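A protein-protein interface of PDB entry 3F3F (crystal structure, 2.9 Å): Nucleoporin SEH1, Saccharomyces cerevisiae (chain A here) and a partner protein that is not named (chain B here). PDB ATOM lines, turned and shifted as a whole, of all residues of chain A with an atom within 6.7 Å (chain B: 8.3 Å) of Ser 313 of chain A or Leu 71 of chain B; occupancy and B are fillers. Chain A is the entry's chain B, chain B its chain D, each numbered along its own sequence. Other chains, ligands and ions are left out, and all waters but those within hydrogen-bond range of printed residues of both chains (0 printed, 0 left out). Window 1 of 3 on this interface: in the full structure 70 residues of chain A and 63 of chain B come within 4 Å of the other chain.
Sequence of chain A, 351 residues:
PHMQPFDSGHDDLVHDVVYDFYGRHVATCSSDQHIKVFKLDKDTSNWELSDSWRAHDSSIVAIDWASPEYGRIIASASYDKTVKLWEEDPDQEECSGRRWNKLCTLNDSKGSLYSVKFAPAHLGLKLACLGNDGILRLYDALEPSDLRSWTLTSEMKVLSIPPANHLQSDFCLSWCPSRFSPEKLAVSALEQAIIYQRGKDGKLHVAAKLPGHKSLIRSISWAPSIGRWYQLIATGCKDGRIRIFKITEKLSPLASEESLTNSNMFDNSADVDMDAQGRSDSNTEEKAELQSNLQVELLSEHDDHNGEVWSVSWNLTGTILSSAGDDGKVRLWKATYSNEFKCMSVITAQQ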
ATOM      1  N   TYR A  19     -17.585  -2.507 -38.482  1.00  0.00           N
ATOM      2  CA  TYR A  19     -16.189  -2.282 -38.832  1.00  0.00           C
ATOM      3  C   TYR A  19     -15.677  -3.338 -39.805  1.00  0.00           C
ATOM      4  O   TYR A  19     -16.137  -4.476 -39.777  1.00  0.00           O
ATOM      5  CB  TYR A  19     -15.330  -2.313 -37.549  1.00  0.00           C
ATOM      6  CG  TYR A  19     -15.308  -1.012 -36.750  1.00  0.00           C
ATOM      7  CD1 TYR A  19     -14.538   0.078 -37.178  1.00  0.00           C
ATOM      8  CD2 TYR A  19     -16.089  -0.854 -35.600  1.00  0.00           C
ATOM      9  CE1 TYR A  19     -14.547   1.284 -36.496  1.00  0.00           C
ATOM     10  CE2 TYR A  19     -16.105   0.354 -34.908  1.00  0.00           C
ATOM     11  CZ  TYR A  19     -15.330   1.420 -35.370  1.00  0.00           C
ATOM     12  OH  TYR A  19     -15.347   2.649 -34.742  1.00  0.00           O
ATOM     13  N   SER A 219     -29.781  -8.156 -28.300  1.00  0.00           N
ATOM     14  CA  SER A 219     -28.477  -8.387 -28.912  1.00  0.00           C
ATOM     15  C   SER A 219     -27.721  -9.553 -28.281  1.00  0.00           C
ATOM     16  O   SER A 219     -27.945  -9.889 -27.115  1.00  0.00           O
ATOM     17  CB  SER A 219     -27.642  -7.102 -28.806  1.00  0.00           C
ATOM     18  OG  SER A 219     -26.337  -7.279 -29.315  1.00  0.00           O
ATOM     19  N   SER A 221     -23.641 -11.701 -28.866  1.00  0.00           N
ATOM     20  CA  SER A 221     -22.427 -11.867 -29.651  1.00  0.00           C
ATOM     21  C   SER A 221     -21.471 -12.830 -28.971  1.00  0.00           C
ATOM     22  O   SER A 221     -21.269 -12.794 -27.757  1.00  0.00           O
ATOM     23  CB  SER A 221     -21.737 -10.530 -29.925  1.00  0.00           C
ATOM     24  OG  SER A 221     -21.264  -9.946 -28.741  1.00  0.00           O
ATOM     25  N   ALA A 234     -22.350 -13.302 -24.861  1.00  0.00           N
ATOM     26  CA  ALA A 234     -23.071 -12.337 -24.051  1.00  0.00           C
ATOM     27  C   ALA A 234     -24.369 -11.913 -24.708  1.00  0.00           C
ATOM     28  O   ALA A 234     -24.471 -11.902 -25.932  1.00  0.00           O
ATOM     29  CB  ALA A 234     -22.188 -11.114 -23.799  1.00  0.00           C
ATOM     30  N   SER A 311     -27.310  -2.850 -27.209  1.00  0.00           N
ATOM     31  CA  SER A 311     -26.111  -3.349 -27.868  1.00  0.00           C
ATOM     32  C   SER A 311     -25.123  -4.039 -26.927  1.00  0.00           C
ATOM     33  O   SER A 311     -24.845  -3.566 -25.822  1.00  0.00           O
ATOM     34  CB  SER A 311     -25.416  -2.193 -28.601  1.00  0.00           C
ATOM     35  OG  SER A 311     -24.154  -2.581 -29.106  1.00  0.00           O
ATOM     36  N   VAL A 312     -24.606  -5.170 -27.387  1.00  0.00           N
ATOM     37  CA  VAL A 312     -23.632  -5.944 -26.641  1.00  0.00           C
ATOM     38  C   VAL A 312     -22.547  -6.269 -27.670  1.00  0.00           C
ATOM     39  O   VAL A 312     -22.828  -6.848 -28.707  1.00  0.00           O
ATOM     40  CB  VAL A 312     -24.304  -7.211 -26.056  1.00  0.00           C
ATOM     41  CG1 VAL A 312     -23.572  -8.461 -26.479  1.00  0.00           C
ATOM     42  CG2 VAL A 312     -24.343  -7.108 -24.548  1.00  0.00           C
ATOM     43  N   SER A 313     -21.313  -5.871 -27.397  1.00  0.00           N
ATOM     44  CA  SER A 313     -20.224  -6.083 -28.346  1.00  0.00           C
ATOM     45  C   SER A 313     -18.936  -6.579 -27.684  1.00  0.00           C
ATOM     46  O   SER A 313     -18.742  -6.387 -26.484  1.00  0.00           O
ATOM     47  CB  SER A 313     -19.969  -4.761 -29.087  1.00  0.00           C
ATOM     48  OG  SER A 313     -18.628  -4.645 -29.532  1.00  0.00           O
ATOM     49  N   TRP A 314     -18.061  -7.222 -28.463  1.00  0.00           N
ATOM     50  CA  TRP A 314     -16.793  -7.715 -27.932  1.00  0.00           C
ATOM     51  C   TRP A 314     -15.555  -7.108 -28.573  1.00  0.00           C
ATOM     52  O   TRP A 314     -15.587  -6.483 -29.632  1.00  0.00           O
ATOM     53  CB  TRP A 314     -16.646  -9.242 -28.049  1.00  0.00           C
ATOM     54  CG  TRP A 314     -17.459 -10.080 -27.098  1.00  0.00           C
ATOM     55  CD1 TRP A 314     -18.606 -10.747 -27.389  1.00  0.00           C
ATOM     56  CD2 TRP A 314     -17.153 -10.402 -25.729  1.00  0.00           C
ATOM     57  NE1 TRP A 314     -19.035 -11.469 -26.304  1.00  0.00           N
ATOM     58  CE2 TRP A 314     -18.161 -11.279 -25.270  1.00  0.00           C
ATOM     59  CE3 TRP A 314     -16.122 -10.044 -24.853  1.00  0.00           C
ATOM     60  CZ2 TRP A 314     -18.173 -11.804 -23.970  1.00  0.00           C
ATOM     61  CZ3 TRP A 314     -16.132 -10.569 -23.554  1.00  0.00           C
ATOM     62  CH2 TRP A 314     -17.155 -11.442 -23.130  1.00  0.00           C
ATOM     63  N   ASN A 315     -14.453  -7.348 -27.879  1.00  0.00           N
ATOM     64  CA  ASN A 315     -13.102  -6.925 -28.225  1.00  0.00           C
ATOM     65  C   ASN A 315     -12.675  -7.749 -29.437  1.00  0.00           C
ATOM     66  O   ASN A 315     -13.425  -8.597 -29.901  1.00  0.00           O
ATOM     67  CB  ASN A 315     -12.203  -7.287 -27.043  1.00  0.00           C
ATOM     68  CG  ASN A 315     -11.101  -6.306 -26.822  1.00  0.00           C
ATOM     69  OD1 ASN A 315     -10.266  -6.506 -25.939  1.00  0.00           O
ATOM     70  ND2 ASN A 315     -11.083  -5.226 -27.610  1.00  0.00           N
ATOM     71  N   LEU A 316     -11.473  -7.520 -29.943  1.00  0.00           N
ATOM     72  CA  LEU A 316     -11.011  -8.324 -31.062  1.00  0.00           C
ATOM     73  C   LEU A 316     -10.363  -9.563 -30.442  1.00  0.00           C
ATOM     74  O   LEU A 316     -10.254 -10.623 -31.070  1.00  0.00           O
ATOM     75  CB  LEU A 316     -10.017  -7.531 -31.921  1.00  0.00           C
ATOM     76  CG  LEU A 316      -8.509  -7.792 -31.889  1.00  0.00           C
ATOM     77  CD1 LEU A 316      -8.172  -9.139 -32.507  1.00  0.00           C
ATOM     78  CD2 LEU A 316      -7.821  -6.679 -32.674  1.00  0.00           C
ATOM     79  N   ILE A 320     -12.465  -7.422 -23.788  1.00  0.00           N
ATOM     80  CA  ILE A 320     -13.364  -6.386 -23.288  1.00  0.00           C
ATOM     81  C   ILE A 320     -14.755  -6.626 -23.877  1.00  0.00           C
ATOM     82  O   ILE A 320     -14.883  -7.002 -25.040  1.00  0.00           O
ATOM     83  CB  ILE A 320     -12.907  -4.956 -23.717  1.00  0.00           C
ATOM     84  CG1 ILE A 320     -11.463  -4.717 -23.287  1.00  0.00           C
ATOM     85  CG2 ILE A 320     -13.853  -3.885 -23.113  1.00  0.00           C
ATOM     86  CD1 ILE A 320     -10.934  -3.404 -23.755  1.00  0.00           C
ATOM     87  N   LEU A 321     -15.785  -6.404 -23.069  1.00  0.00           N
ATOM     88  CA  LEU A 321     -17.159  -6.575 -23.507  1.00  0.00           C
ATOM     89  C   LEU A 321     -17.866  -5.261 -23.309  1.00  0.00           C
ATOM     90  O   LEU A 321     -17.712  -4.634 -22.273  1.00  0.00           O
ATOM     91  CB  LEU A 321     -17.876  -7.632 -22.673  1.00  0.00           C
ATOM     92  CG  LEU A 321     -19.400  -7.661 -22.845  1.00  0.00           C
ATOM     93  CD1 LEU A 321     -19.782  -8.082 -24.266  1.00  0.00           C
ATOM     94  CD2 LEU A 321     -19.985  -8.617 -21.824  1.00  0.00           C
ATOM     95  N   SER A 322     -18.660  -4.853 -24.290  1.00  0.00           N
ATOM     96  CA  SER A 322     -19.388  -3.594 -24.182  1.00  0.00           C
ATOM     97  C   SER A 322     -20.897  -3.804 -24.139  1.00  0.00           C
ATOM     98  O   SER A 322     -21.425  -4.783 -24.665  1.00  0.00           O
ATOM     99  CB  SER A 322     -19.048  -2.685 -25.362  1.00  0.00           C
ATOM    100  OG  SER A 322     -19.587  -3.213 -26.564  1.00  0.00           O
ATOM    101  N   SER A 323     -21.577  -2.867 -23.495  1.00  0.00           N
ATOM    102  CA  SER A 323     -23.028  -2.890 -23.383  1.00  0.00           C
ATOM    103  C   SER A 323     -23.533  -1.445 -23.411  1.00  0.00           C
ATOM    104  O   SER A 323     -22.901  -0.541 -22.849  1.00  0.00           O
ATOM    105  CB  SER A 323     -23.460  -3.563 -22.081  1.00  0.00           C
ATOM    106  OG  SER A 323     -23.015  -2.839 -20.944  1.00  0.00           O
ATOM    107  N   ALA A 324     -24.661  -1.231 -24.085  1.00  0.00           N
ATOM    108  CA  ALA A 324     -25.268   0.097 -24.179  1.00  0.00           C
ATOM    109  C   ALA A 324     -26.775  -0.057 -23.981  1.00  0.00           C
ATOM    110  O   ALA A 324     -27.347  -1.092 -24.334  1.00  0.00           O
ATOM    111  CB  ALA A 324     -24.965   0.723 -25.536  1.00  0.00           C
ATOM    112  N   VAL A 330     -22.679   3.653 -22.105  1.00  0.00           N
ATOM    113  CA  VAL A 330     -21.944   2.505 -22.622  1.00  0.00           C
ATOM    114  C   VAL A 330     -21.030   2.034 -21.492  1.00  0.00           C
ATOM    115  O   VAL A 330     -20.347   2.848 -20.866  1.00  0.00           O
ATOM    116  CB  VAL A 330     -21.069   2.890 -23.842  1.00  0.00           C
ATOM    117  CG1 VAL A 330     -20.208   1.707 -24.253  1.00  0.00           C
ATOM    118  CG2 VAL A 330     -21.955   3.330 -25.001  1.00  0.00           C
ATOM    119  N   LEU A 332     -17.975  -0.797 -20.272  1.00  0.00           N
ATOM    120  CA  LEU A 332     -16.947  -1.729 -20.713  1.00  0.00           C
ATOM    121  C   LEU A 332     -16.690  -2.685 -19.553  1.00  0.00           C
ATOM    122  O   LEU A 332     -16.576  -2.257 -18.414  1.00  0.00           O
ATOM    123  CB  LEU A 332     -15.684  -0.962 -21.113  1.00  0.00           C
ATOM    124  CG  LEU A 332     -15.944   0.051 -22.232  1.00  0.00           C
ATOM    125  CD1 LEU A 332     -14.693   0.840 -22.545  1.00  0.00           C
ATOM    126  CD2 LEU A 332     -16.416  -0.688 -23.460  1.00  0.00           C
ATOM    127  N   LYS B  68     -26.525   2.276 -29.130  1.00  0.00           N
ATOM    128  CA  LYS B  68     -25.819   1.084 -29.554  1.00  0.00           C
ATOM    129  C   LYS B  68     -24.347   1.421 -29.635  1.00  0.00           C
ATOM    130  O   LYS B  68     -23.973   2.542 -29.990  1.00  0.00           O
ATOM    131  CB  LYS B  68     -26.385   0.605 -30.896  1.00  0.00           C
ATOM    132  CG  LYS B  68     -27.861   0.185 -30.782  1.00  0.00           C
ATOM    133  CD  LYS B  68     -28.464  -0.262 -32.103  1.00  0.00           C
ATOM    134  CE  LYS B  68     -29.911  -0.736 -31.908  1.00  0.00           C
ATOM    135  NZ  LYS B  68     -30.525  -1.287 -33.172  1.00  0.00           N
ATOM    136  N   PHE B  69     -23.513   0.452 -29.279  1.00  0.00           N
ATOM    137  CA  PHE B  69     -22.072   0.661 -29.260  1.00  0.00           C
ATOM    138  C   PHE B  69     -21.332  -0.558 -29.781  1.00  0.00           C
ATOM    139  O   PHE B  69     -21.655  -1.697 -29.416  1.00  0.00           O
ATOM    140  CB  PHE B  69     -21.617   0.945 -27.819  1.00  0.00           C
ATOM    141  CG  PHE B  69     -20.153   1.253 -27.689  1.00  0.00           C
ATOM    142  CD1 PHE B  69     -19.655   2.498 -28.067  1.00  0.00           C
ATOM    143  CD2 PHE B  69     -19.264   0.293 -27.203  1.00  0.00           C
ATOM    144  CE1 PHE B  69     -18.290   2.785 -27.967  1.00  0.00           C
ATOM    145  CE2 PHE B  69     -17.903   0.567 -27.099  1.00  0.00           C
ATOM    146  CZ  PHE B  69     -17.417   1.818 -27.484  1.00  0.00           C
ATOM    147  N   LYS B  70     -20.339  -0.326 -30.635  1.00  0.00           N
ATOM    148  CA  LYS B  70     -19.550  -1.436 -31.154  1.00  0.00           C
ATOM    149  C   LYS B  70     -18.061  -1.200 -31.031  1.00  0.00           C
ATOM    150  O   LYS B  70     -17.535  -0.236 -31.587  1.00  0.00           O
ATOM    151  CB  LYS B  70     -19.913  -1.731 -32.605  1.00  0.00           C
ATOM    152  CG  LYS B  70     -21.237  -2.442 -32.721  1.00  0.00           C
ATOM    153  CD  LYS B  70     -21.392  -3.101 -34.063  1.00  0.00           C
ATOM    154  CE  LYS B  70     -22.640  -3.970 -34.103  1.00  0.00           C
ATOM    155  NZ  LYS B  70     -22.785  -4.681 -35.413  1.00  0.00           N
ATOM    156  N   LEU B  71     -17.404  -2.080 -30.278  1.00  0.00           N
ATOM    157  CA  LEU B  71     -15.960  -2.016 -30.069  1.00  0.00           C
ATOM    158  C   LEU B  71     -15.247  -2.332 -31.390  1.00  0.00           C
ATOM    159  O   LEU B  71     -15.534  -3.345 -32.037  1.00  0.00           O
ATOM    160  CB  LEU B  71     -15.521  -3.034 -29.001  1.00  0.00           C
ATOM    161  CG  LEU B  71     -15.924  -2.826 -27.541  1.00  0.00           C
ATOM    162  CD1 LEU B  71     -15.632  -4.083 -26.722  1.00  0.00           C
ATOM    163  CD2 LEU B  71     -15.166  -1.633 -26.998  1.00  0.00           C
ATOM    164  N   GLY B  72     -14.309  -1.466 -31.772  1.00  0.00           N
ATOM    165  CA  GLY B  72     -13.574  -1.646 -33.015  1.00  0.00           C
ATOM    166  C   GLY B  72     -12.282  -2.434 -32.914  1.00  0.00           C
ATOM    167  O   GLY B  72     -11.753  -2.637 -31.821  1.00  0.00           O
ATOM    168  N   PRO B  73     -11.744  -2.898 -34.051  1.00  0.00           N
ATOM    169  CA  PRO B  73     -10.498  -3.671 -34.084  1.00  0.00           C
ATOM    170  C   PRO B  73      -9.333  -2.872 -33.511  1.00  0.00           C
ATOM    171  O   PRO B  73      -8.285  -3.432 -33.175  1.00  0.00           O
ATOM    172  CB  PRO B  73     -10.318  -3.960 -35.571  1.00  0.00           C
ATOM    173  CG  PRO B  73     -11.718  -4.015 -36.081  1.00  0.00           C
ATOM    174  CD  PRO B  73     -12.330  -2.817 -35.399  1.00  0.00           C
ATOM    175  N   LEU B  74      -9.540  -1.563 -33.412  1.00  0.00           N
ATOM    176  CA  LEU B  74      -8.546  -0.641 -32.885  1.00  0.00           C
ATOM    177  C   LEU B  74      -9.031   0.015 -31.585  1.00  0.00           C
ATOM    178  O   LEU B  74     -10.069   0.669 -31.575  1.00  0.00           O
ATOM    179  CB  LEU B  74      -8.247   0.429 -33.940  1.00  0.00           C
ATOM    180  CG  LEU B  74      -7.528  -0.093 -35.195  1.00  0.00           C
ATOM    181  CD1 LEU B  74      -7.477   0.979 -36.257  1.00  0.00           C
ATOM    182  CD2 LEU B  74      -6.104  -0.521 -34.838  1.00  0.00           C
ATOM    183  N   SER B  75      -8.280  -0.172 -30.496  1.00  0.00           N
ATOM    184  CA  SER B  75      -8.616   0.400 -29.184  1.00  0.00           C
ATOM    185  C   SER B  75      -9.038   1.862 -29.266  1.00  0.00           C
ATOM    186  O   SER B  75      -9.989   2.289 -28.610  1.00  0.00           O
ATOM    187  CB  SER B  75      -7.409   0.335 -28.235  1.00  0.00           C
ATOM    188  OG  SER B  75      -7.000  -0.990 -27.938  1.00  0.00           O
ATOM    189  N   GLN B  77     -10.379   3.464 -31.727  1.00  0.00           N
ATOM    190  CA  GLN B  77     -11.437   3.765 -32.690  1.00  0.00           C
ATOM    191  C   GLN B  77     -12.638   2.846 -32.579  1.00  0.00           C
ATOM    192  O   GLN B  77     -12.696   1.806 -33.237  1.00  0.00           O
ATOM    193  CB  GLN B  77     -10.908   3.697 -34.112  1.00  0.00           C
ATOM    194  CG  GLN B  77     -11.633   4.659 -34.991  1.00  0.00           C
ATOM    195  CD  GLN B  77     -11.086   6.057 -34.850  1.00  0.00           C
ATOM    196  OE1 GLN B  77     -11.810   7.048 -34.992  1.00  0.00           O
ATOM    197  NE2 GLN B  77      -9.791   6.149 -34.583  1.00  0.00           N
ATOM    198  N   ASN B  78     -13.580   3.236 -31.727  1.00  0.00           N
ATOM    199  CA  ASN B  78     -14.814   2.491 -31.520  1.00  0.00           C
ATOM    200  C   ASN B  78     -15.936   3.370 -32.067  1.00  0.00           C
ATOM    201  O   ASN B  78     -15.666   4.389 -32.716  1.00  0.00           O
ATOM    202  CB  ASN B  78     -15.007   2.200 -30.034  1.00  0.00           C
ATOM    203  CG  ASN B  78     -13.872   1.374 -29.463  1.00  0.00           C
ATOM    204  OD1 ASN B  78     -13.804   0.160 -29.655  1.00  0.00           O
ATOM    205  ND2 ASN B  78     -12.958   2.038 -28.773  1.00  0.00           N
ATOM    206  N   MET B  79     -17.184   2.997 -31.815  1.00  0.00           N
ATOM    207  CA  MET B  79     -18.282   3.783 -32.350  1.00  0.00           C
ATOM    208  C   MET B  79     -19.589   3.591 -31.601  1.00  0.00           C
ATOM    209  O   MET B  79     -19.974   2.467 -31.232  1.00  0.00           O
ATOM    210  CB  MET B  79     -18.491   3.409 -33.818  1.00  0.00           C
ATOM    211  CG  MET B  79     -19.296   4.396 -34.644  1.00  0.00           C
ATOM    212  SD  MET B  79     -18.308   5.837 -35.041  1.00  0.00           S
ATOM    213  CE  MET B  79     -17.167   5.192 -36.277  1.00  0.00           C
ATOM    214  N   ALA B  80     -20.271   4.712 -31.396  1.00  0.00           N
ATOM    215  CA  ALA B  80     -21.567   4.735 -30.726  1.00  0.00           C
ATOM    216  C   ALA B  80     -22.559   5.392 -31.691  1.00  0.00           C
ATOM    217  O   ALA B  80     -22.176   6.247 -32.493  1.00  0.00           O
ATOM    218  CB  ALA B  80     -21.474   5.539 -29.431  1.00  0.00           C
ATOM    219  N   VAL B  93     -15.765   6.806 -30.475  1.00  0.00           N
ATOM    220  CA  VAL B  93     -15.327   6.827 -29.087  1.00  0.00           C
ATOM    221  C   VAL B  93     -14.064   6.001 -28.906  1.00  0.00           C
ATOM    222  O   VAL B  93     -13.970   4.895 -29.436  1.00  0.00           O
ATOM    223  CB  VAL B  93     -16.426   6.219 -28.173  1.00  0.00           C
ATOM    224  CG1 VAL B  93     -15.936   6.116 -26.738  1.00  0.00           C
ATOM    225  CG2 VAL B  93     -17.680   7.066 -28.247  1.00  0.00           C
ATOM    226  N   ARG B  94     -13.088   6.531 -28.172  1.00  0.00           N
ATOM    227  CA  ARG B  94     -11.884   5.753 -27.910  1.00  0.00           C
ATOM    228  C   ARG B  94     -11.918   5.302 -26.469  1.00  0.00           C
ATOM    229  O   ARG B  94     -12.380   6.031 -25.596  1.00  0.00           O
ATOM    230  CB  ARG B  94     -10.613   6.546 -28.194  1.00  0.00           C
ATOM    231  CG  ARG B  94     -10.569   7.923 -27.642  1.00  0.00           C
ATOM    232  CD  ARG B  94      -9.285   8.559 -28.122  1.00  0.00           C
ATOM    233  NE  ARG B  94      -8.134   8.108 -27.345  1.00  0.00           N
ATOM    234  CZ  ARG B  94      -6.885   8.091 -27.798  1.00  0.00           C
ATOM    235  NH1 ARG B  94      -6.625   8.491 -29.035  1.00  0.00           N
ATOM    236  NH2 ARG B  94      -5.896   7.693 -27.007  1.00  0.00           N
ATOM    237  N   ILE B  95     -11.437   4.088 -26.228  1.00  0.00           N
ATOM    238  CA  ILE B  95     -11.457   3.517 -24.889  1.00  0.00           C
ATOM    239  C   ILE B  95     -10.823   4.378 -23.810  1.00  0.00           C
ATOM    240  O   ILE B  95      -9.658   4.779 -23.909  1.00  0.00           O
ATOM    241  CB  ILE B  95     -10.810   2.118 -24.849  1.00  0.00           C
ATOM    242  CG1 ILE B  95     -11.572   1.183 -25.788  1.00  0.00           C
ATOM    243  CG2 ILE B  95     -10.843   1.568 -23.423  1.00  0.00           C
ATOM    244  CD1 ILE B  95     -11.225  -0.262 -25.630  1.00  0.00           C
ATOM    245  N   PRO B  96     -11.601   4.668 -22.752  1.00  0.00           N
ATOM    246  CA  PRO B  96     -11.202   5.477 -21.602  1.00  0.00           C
ATOM    247  C   PRO B  96      -9.805   5.146 -21.107  1.00  0.00           C
ATOM    248  O   PRO B  96      -9.468   3.977 -20.875  1.00  0.00           O
ATOM    249  CB  PRO B  96     -12.281   5.146 -20.578  1.00  0.00           C
ATOM    250  CG  PRO B  96     -13.493   5.034 -21.442  1.00  0.00           C
ATOM    251  CD  PRO B  96     -12.980   4.172 -22.577  1.00  0.00           C
ATOM    252  N   SER B 475      -4.617  -4.641 -29.990  1.00  0.00           N
ATOM    253  CA  SER B 475      -5.642  -3.721 -30.480  1.00  0.00           C
ATOM    254  C   SER B 475      -5.121  -2.289 -30.520  1.00  0.00           C
ATOM    255  O   SER B 475      -5.816  -1.392 -30.996  1.00  0.00           O
ATOM    256  CB  SER B 475      -6.888  -3.759 -29.599  1.00  0.00           C
ATOM    257  OG  SER B 475      -7.607  -4.962 -29.782  1.00  0.00           O
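The side-chain hydroxyl of Tyr 19 of chain A is in hydrogen-bond range of the backbone carbonyl oxygen of Gln 77 of chain B (3.2 Å). The side-chain hydroxyl (OH) of Tyr 19 of chain A lies within hydrogen-bond range of the backbone carbonyl oxygen (O) of Asn 78 of chain B (2.7 Å). OH of Tyr 19 of chain A sits close to N of Met 79 of chain B, at 3.5 Å. The side-chain hydroxyl (OG) of Ser 311 of chain A is in hydrogen-bond range of the backbone carbonyl oxygen (O) of Phe 69 of chain B, 2.7 Å away. The backbone NH (N) of Leu 71 of chain B lies within hydrogen-bond range of the side-chain hydroxyl (OG) of Ser 313 of chain A (2.9 Å).
Printed residues of chain B that touch a printed residue of chain A: Lys 68, Phe 69, Lys 70, Leu 71, Gly 72, Pro 73, Gln 77, Asn 78, Met 79, Ile 95, Pro 96 and Ser 475. Hydrophobic or aromatic side chains of chain B within 4 Å of the printed part of chain A: Phe 69, Leu 71, Pro 73, Met 79, Ile 95 and Pro 96. Among the printed residues, 22 pairs touch across the chains. Among the printed residues, no Asp or Glu carboxylate lies within 4 Å of a Lys or Arg side-chain nitrogen of the other chain.
Among the printed residues, pairs that only touch across the chains: Leu 316 of chain A with Pro 73 of chain B (3.3 Å), Leu 316 of chain A with Ser 475 of chain B (3.4 Å), Val 330 of chain A with Phe 69 of chain B (3.4 Å), Ser 311 of chain A with Lys 68 of chain B (3.4 Å), Ile 320 of chain A with Leu 71 of chain B (3.5 Å), Trp 314 of chain A with Leu 71 of chain B (3.5 Å), Ser 322 of chain A with Phe 69 of chain B (3.5 Å), Ser 313 of chain A with Phe 69 of chain B (3.5 Å), Asn 315 of chain A with Leu 71 of chain B (3.7 Å), Tyr 19 of chain A with Lys 70 of chain B (3.7 Å), Ile 320 of chain A with Ile 95 of chain B (3.7 Å), Tyr 19 of chain A with Gly 72 of chain B (3.7 Å), Ser 313 of chain A with Lys 70 of chain B (3.7 Å), Tyr 19 of chain A with Pro 73 of chain B (3.7 Å), Leu 332 of chain A with Pro 96 of chain B (3.7 Å), Ser 322 of chain A with Leu 71 of chain B (3.8 Å) and Leu 332 of chain A with Leu 71 of chain B (3.9 Å).
Ser 313 of chain A touches three residues of chain B. Leu 71 of chain B touches just these residues of chain A: Ser 313 (2.9 Å), Trp 314 (3.5 Å), Asn 315 (3.7 Å), Ile 320 (3.5 Å), Ser 322 (3.8 Å) and Leu 332 (3.9 Å). Ser 322 of chain A touches two residues of chain B. Of the printed residues of chain B, Asn 315 of chain A touches Leu 71 (3.7 Å). Of the printed residues of chain A, Phe 69 of chain B touches Ser 311, Ser 313, Ser 322 and Val 330. Of the printed residues of chain B, Trp 314 of chain A touches Leu 71 (3.5 Å). Of the printed residues of chain B, Leu 316 of chain A touches Pro 73 (3.3 Å) and Ser 475 (3.4 Å). Of the printed residues of chain B, Ser 311 of chain A touches Lys 68 (3.4 Å) and Phe 69 (2.7 Å). The nearest residue of chain A that does not touch Leu 71 of chain B is Leu 321 of chain A (4.2 Å). The nearest printed residue of chain B that does not touch Asn 315 of chain A is Ser 475 of chain B (4.1 Å).
The backbone carbonyl oxygen (O) of Ser 221 of chain A is in hydrogen-bond range of the indole nitrogen (NE1) of Trp 314 of chain A, at 3.0 Å. O of Ser 311 of chain A is in hydrogen-bond range of N of Ala 324 of chain A (2.9 Å). O of Ile 320 of chain A is in hydrogen-bond range of N of Asn 315 of chain A, 2.9 Å away. The backbone NH of Lys 70 of chain B sits at hydrogen-bond distance from the backbone carbonyl oxygen of Met 79 of chain B, at 2.9 Å. The backbone carbonyl oxygen (O) of Ser 475 of chain B lies within hydrogen-bond range of the backbone NH (N) of Ser 75 of chain B, 2.8 Å away. The backbone NH (N) of Asn 78 of chain B sits at hydrogen-bond distance from the backbone carbonyl oxygen (O) of Val 93 of chain B (2.9 Å).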
